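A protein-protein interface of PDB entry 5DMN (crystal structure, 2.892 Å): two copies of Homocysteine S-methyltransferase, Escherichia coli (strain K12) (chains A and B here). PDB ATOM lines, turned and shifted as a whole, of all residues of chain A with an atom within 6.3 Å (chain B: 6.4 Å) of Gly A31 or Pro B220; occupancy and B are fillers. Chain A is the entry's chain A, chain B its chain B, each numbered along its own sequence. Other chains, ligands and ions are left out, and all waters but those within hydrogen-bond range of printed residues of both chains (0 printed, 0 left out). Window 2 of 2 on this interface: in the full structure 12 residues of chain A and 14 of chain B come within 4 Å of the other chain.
No position is printed for both chains.
Among the printed residues, merely in contact across the chains: Ala A29 with Pro B220, Ala A29 with Gln B221, Arg A30 with Pro B220 and Gly A31 with Pro B220.
Printed residues of chain A that touch a printed residue of chain B: Ala A29, Arg A30 and Gly A31. Hydrophobic or aromatic side chains of chain B that line the printed part of chain A: Tyr B219 and Pro B220. Among the printed residues, 6 pairs touch across the chains.
Printed residues of chain B within 4 Å of Ala A29: Pro B220 and Gln B221. Printed residues of chain B within 4 Å of Gly A31: Pro B220 (3.97 Å). Arg B190 touches none of the printed residues of chain A. Of the printed residues of chain A, Gly B218 touches Arg A30 (2.6 Å). Printed residues of chain A within 4 Å of Tyr B219: Arg A30. Pro B220 touches just these residues of chain A: Ala A29 (3.5 Å), Arg A30 (3.6 Å) and Gly A31 (3.97 Å). Printed residues of chain A within 4 Å of Gln B221: Ala A29 (3.6 Å). Val B222 touches none of the printed residues of chain A. The nearest residue of chain B that does not touch Gly A31 is Gly B218 (6.2 Å).
NE of Arg A30 lies within hydrogen-bond range of O of Gly B218, 2.6 Å away. The guanidinium group (NH2) of Arg A30 lies close to the side-chain hydroxyl (OH) of Tyr B219 (3.2 Å).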
ATOM      1  N   GLU A  26      13.495   8.159  -9.531  1.00  0.00           N
ATOM      2  CA  GLU A  26      13.683   8.912 -10.765  1.00  0.00           C
ATOM      3  C   GLU A  26      14.827   9.908 -10.636  1.00  0.00           C
ATOM      4  O   GLU A  26      15.579  10.135 -11.586  1.00  0.00           O
ATOM      5  CB  GLU A  26      12.398   9.648 -11.133  1.00  0.00           C
ATOM      6  CG  GLU A  26      11.370   8.809 -11.864  1.00  0.00           C
ATOM      7  CD  GLU A  26      11.600   8.782 -13.352  1.00  0.00           C
ATOM      8  OE1 GLU A  26      12.192   9.754 -13.873  1.00  0.00           O
ATOM      9  OE2 GLU A  26      11.167   7.807 -14.006  1.00  0.00           O
ATOM     10  N   LEU A  27      14.947  10.511  -9.457  1.00  0.00           N
ATOM     11  CA  LEU A  27      16.000  11.484  -9.210  1.00  0.00           C
ATOM     12  C   LEU A  27      17.375  10.831  -9.181  1.00  0.00           C
ATOM     13  O   LEU A  27      18.347  11.392  -9.682  1.00  0.00           O
ATOM     14  CB  LEU A  27      15.747  12.224  -7.903  1.00  0.00           C
ATOM     15  CG  LEU A  27      14.570  13.192  -7.967  1.00  0.00           C
ATOM     16  CD1 LEU A  27      14.431  13.952  -6.652  1.00  0.00           C
ATOM     17  CD2 LEU A  27      14.712  14.137  -9.158  1.00  0.00           C
ATOM     18  N   GLU A  28      17.452   9.642  -8.593  1.00  0.00           N
ATOM     19  CA  GLU A  28      18.696   8.883  -8.583  1.00  0.00           C
ATOM     20  C   GLU A  28      19.152   8.596 -10.010  1.00  0.00           C
ATOM     21  O   GLU A  28      20.345   8.621 -10.303  1.00  0.00           O
ATOM     22  CB  GLU A  28      18.532   7.573  -7.809  1.00  0.00           C
ATOM     23  CG  GLU A  28      18.478   7.735  -6.298  1.00  0.00           C
ATOM     24  CD  GLU A  28      18.266   6.412  -5.578  1.00  0.00           C
ATOM     25  OE1 GLU A  28      17.447   6.369  -4.630  1.00  0.00           O
ATOM     26  OE2 GLU A  28      18.914   5.413  -5.964  1.00  0.00           O
ATOM     27  N   ALA A  29      18.196   8.327 -10.893  1.00  0.00           N
ATOM     28  CA  ALA A  29      18.505   8.054 -12.292  1.00  0.00           C
ATOM     29  C   ALA A  29      19.137   9.267 -12.957  1.00  0.00           C
ATOM     30  O   ALA A  29      19.994   9.128 -13.826  1.00  0.00           O
ATOM     31  CB  ALA A  29      17.251   7.629 -13.047  1.00  0.00           C
ATOM     32  N   ARG A  30      18.711  10.456 -12.546  1.00  0.00           N
ATOM     33  CA  ARG A  30      19.226  11.690 -13.125  1.00  0.00           C
ATOM     34  C   ARG A  30      20.465  12.212 -12.393  1.00  0.00           C
ATOM     35  O   ARG A  30      20.996  13.263 -12.744  1.00  0.00           O
ATOM     36  CB  ARG A  30      18.133  12.761 -13.132  1.00  0.00           C
ATOM     37  CG  ARG A  30      17.002  12.475 -14.115  1.00  0.00           C
ATOM     38  CD  ARG A  30      17.506  12.504 -15.551  1.00  0.00           C
ATOM     39  NE  ARG A  30      18.046  13.813 -15.911  1.00  0.00           N
ATOM     40  CZ  ARG A  30      17.374  14.743 -16.583  1.00  0.00           C
ATOM     41  NH1 ARG A  30      17.950  15.906 -16.857  1.00  0.00           N
ATOM     42  NH2 ARG A  30      16.135  14.510 -16.992  1.00  0.00           N
ATOM     43  N   GLY A  31      20.924  11.475 -11.383  1.00  0.00           N
ATOM     44  CA  GLY A  31      22.160  11.799 -10.689  1.00  0.00           C
ATOM     45  C   GLY A  31      22.001  12.662  -9.448  1.00  0.00           C
ATOM     46  O   GLY A  31      22.797  13.568  -9.213  1.00  0.00           O
ATOM     47  N   CYS A  32      20.968  12.384  -8.657  1.00  0.00           N
ATOM     48  CA  CYS A  32      20.698  13.114  -7.414  1.00  0.00           C
ATOM     49  C   CYS A  32      21.139  12.387  -6.144  1.00  0.00           C
ATOM     50  O   CYS A  32      21.337  11.173  -6.145  1.00  0.00           O
ATOM     51  CB  CYS A  32      19.209  13.428  -7.308  1.00  0.00           C
ATOM     52  SG  CYS A  32      18.717  14.879  -8.238  1.00  0.00           S
ATOM     53  N   ASN A  33      21.273  13.144  -5.057  1.00  0.00           N
ATOM     54  CA  ASN A  33      21.568  12.579  -3.742  1.00  0.00           C
ATOM     55  C   ASN A  33      20.335  12.568  -2.838  1.00  0.00           C
ATOM     56  O   ASN A  33      19.756  11.515  -2.565  1.00  0.00           O
ATOM     57  CB  ASN A  33      22.684  13.368  -3.055  1.00  0.00           C
ATOM     58  CG  ASN A  33      24.063  12.929  -3.492  1.00  0.00           C
ATOM     59  OD1 ASN A  33      24.219  11.912  -4.173  1.00  0.00           O
ATOM     60  ND2 ASN A  33      25.078  13.693  -3.098  1.00  0.00           N
ATOM     61  N   LEU A  50      14.196  19.109 -12.573  1.00  0.00           N
ATOM     62  CA  LEU A  50      14.134  17.653 -12.448  1.00  0.00           C
ATOM     63  C   LEU A  50      12.820  17.196 -11.831  1.00  0.00           C
ATOM     64  O   LEU A  50      12.171  16.278 -12.331  1.00  0.00           O
ATOM     65  CB  LEU A  50      15.297  17.133 -11.604  1.00  0.00           C
ATOM     66  CG  LEU A  50      16.656  17.068 -12.304  1.00  0.00           C
ATOM     67  CD1 LEU A  50      17.687  16.385 -11.418  1.00  0.00           C
ATOM     68  CD2 LEU A  50      16.534  16.356 -13.641  1.00  0.00           C
ATOM     69  N   ARG B 190      21.546   0.606 -18.017  1.00  0.00           N
ATOM     70  CA  ARG B 190      22.576   1.420 -18.661  1.00  0.00           C
ATOM     71  C   ARG B 190      22.445   1.280 -20.169  1.00  0.00           C
ATOM     72  O   ARG B 190      22.102   0.213 -20.675  1.00  0.00           O
ATOM     73  CB  ARG B 190      23.977   1.001 -18.214  1.00  0.00           C
ATOM     74  CG  ARG B 190      24.251   1.226 -16.746  1.00  0.00           C
ATOM     75  CD  ARG B 190      24.134   2.694 -16.403  1.00  0.00           C
ATOM     76  NE  ARG B 190      24.475   2.948 -15.008  1.00  0.00           N
ATOM     77  CZ  ARG B 190      23.611   2.850 -14.002  1.00  0.00           C
ATOM     78  NH1 ARG B 190      22.352   2.506 -14.237  1.00  0.00           N
ATOM     79  NH2 ARG B 190      24.007   3.102 -12.762  1.00  0.00           N
ATOM     80  N   LEU B 216      21.166  14.565 -23.862  1.00  0.00           N
ATOM     81  CA  LEU B 216      21.565  13.289 -23.288  1.00  0.00           C
ATOM     82  C   LEU B 216      22.614  13.456 -22.192  1.00  0.00           C
ATOM     83  O   LEU B 216      22.846  12.541 -21.403  1.00  0.00           O
ATOM     84  CB  LEU B 216      22.091  12.363 -24.388  1.00  0.00           C
ATOM     85  CG  LEU B 216      21.041  11.922 -25.412  1.00  0.00           C
ATOM     86  CD1 LEU B 216      21.668  11.111 -26.538  1.00  0.00           C
ATOM     87  CD2 LEU B 216      19.918  11.135 -24.744  1.00  0.00           C
ATOM     88  N   ALA B 217      23.226  14.634 -22.127  1.00  0.00           N
ATOM     89  CA  ALA B 217      24.234  14.909 -21.109  1.00  0.00           C
ATOM     90  C   ALA B 217      23.589  15.002 -19.732  1.00  0.00           C
ATOM     91  O   ALA B 217      24.234  14.768 -18.712  1.00  0.00           O
ATOM     92  CB  ALA B 217      24.983  16.182 -21.433  1.00  0.00           C
ATOM     93  N   GLY B 218      22.306  15.344 -19.714  1.00  0.00           N
ATOM     94  CA  GLY B 218      21.549  15.372 -18.480  1.00  0.00           C
ATOM     95  C   GLY B 218      21.054  14.004 -18.038  1.00  0.00           C
ATOM     96  O   GLY B 218      20.339  13.895 -17.045  1.00  0.00           O
ATOM     97  N   TYR B 219      21.415  12.958 -18.776  1.00  0.00           N
ATOM     98  CA  TYR B 219      20.958  11.605 -18.458  1.00  0.00           C
ATOM     99  C   TYR B 219      22.117  10.634 -18.221  1.00  0.00           C
ATOM    100  O   TYR B 219      22.563   9.952 -19.147  1.00  0.00           O
ATOM    101  CB  TYR B 219      20.057  11.075 -19.574  1.00  0.00           C
ATOM    102  CG  TYR B 219      18.720  11.773 -19.664  1.00  0.00           C
ATOM    103  CD1 TYR B 219      17.585  11.214 -19.093  1.00  0.00           C
ATOM    104  CD2 TYR B 219      18.592  12.992 -20.318  1.00  0.00           C
ATOM    105  CE1 TYR B 219      16.358  11.844 -19.169  1.00  0.00           C
ATOM    106  CE2 TYR B 219      17.368  13.632 -20.399  1.00  0.00           C
ATOM    107  CZ  TYR B 219      16.255  13.052 -19.823  1.00  0.00           C
ATOM    108  OH  TYR B 219      15.034  13.685 -19.899  1.00  0.00           O
ATOM    109  N   PRO B 220      22.576  10.539 -16.964  1.00  0.00           N
ATOM    110  CA  PRO B 220      23.705   9.702 -16.538  1.00  0.00           C
ATOM    111  C   PRO B 220      23.586   8.236 -16.949  1.00  0.00           C
ATOM    112  O   PRO B 220      24.600   7.552 -17.065  1.00  0.00           O
ATOM    113  CB  PRO B 220      23.673   9.821 -15.014  1.00  0.00           C
ATOM    114  CG  PRO B 220      22.995  11.101 -14.751  1.00  0.00           C
ATOM    115  CD  PRO B 220      21.969  11.251 -15.828  1.00  0.00           C
ATOM    116  N   GLN B 221      22.371   7.746 -17.154  1.00  0.00           N
ATOM    117  CA  GLN B 221      22.209   6.352 -17.550  1.00  0.00           C
ATOM    118  C   GLN B 221      22.754   6.133 -18.951  1.00  0.00           C
ATOM    119  O   GLN B 221      23.220   5.046 -19.275  1.00  0.00           O
ATOM    120  CB  GLN B 221      20.752   5.928 -17.469  1.00  0.00           C
ATOM    121  CG  GLN B 221      20.348   5.464 -16.087  1.00  0.00           C
ATOM    122  CD  GLN B 221      18.855   5.284 -15.965  1.00  0.00           C
ATOM    123  OE1 GLN B 221      18.080   6.196 -16.265  1.00  0.00           O
ATOM    124  NE2 GLN B 221      18.437   4.095 -15.543  1.00  0.00           N
ATOM    125  N   VAL B 222      22.713   7.178 -19.770  1.00  0.00           N
ATOM    126  CA  VAL B 222      23.340   7.144 -21.085  1.00  0.00           C
ATOM    127  C   VAL B 222      24.859   7.193 -20.935  1.00  0.00           C
ATOM    128  O   VAL B 222      25.426   8.229 -20.595  1.00  0.00           O
ATOM    129  CB  VAL B 222      22.859   8.311 -21.960  1.00  0.00           C
ATOM    130  CG1 VAL B 222      23.655   8.372 -23.259  1.00  0.00           C
ATOM    131  CG2 VAL B 222      21.352   8.200 -22.216  1.00  0.00           C
ATOM    132  N   VAL B 223      25.512   6.062 -21.184  1.00  0.00           N
ATOM    133  CA  VAL B 223      26.931   5.922 -20.887  1.00  0.00           C
ATOM    134  C   VAL B 223      27.824   5.978 -22.119  1.00  0.00           C
ATOM    135  O   VAL B 223      29.049   5.886 -22.000  1.00  0.00           O
ATOM    136  CB  VAL B 223      27.212   4.603 -20.140  1.00  0.00           C
ATOM    137  CG1 VAL B 223      26.527   4.605 -18.783  1.00  0.00           C
ATOM    138  CG2 VAL B 223      26.771   3.411 -20.973  1.00  0.00           C
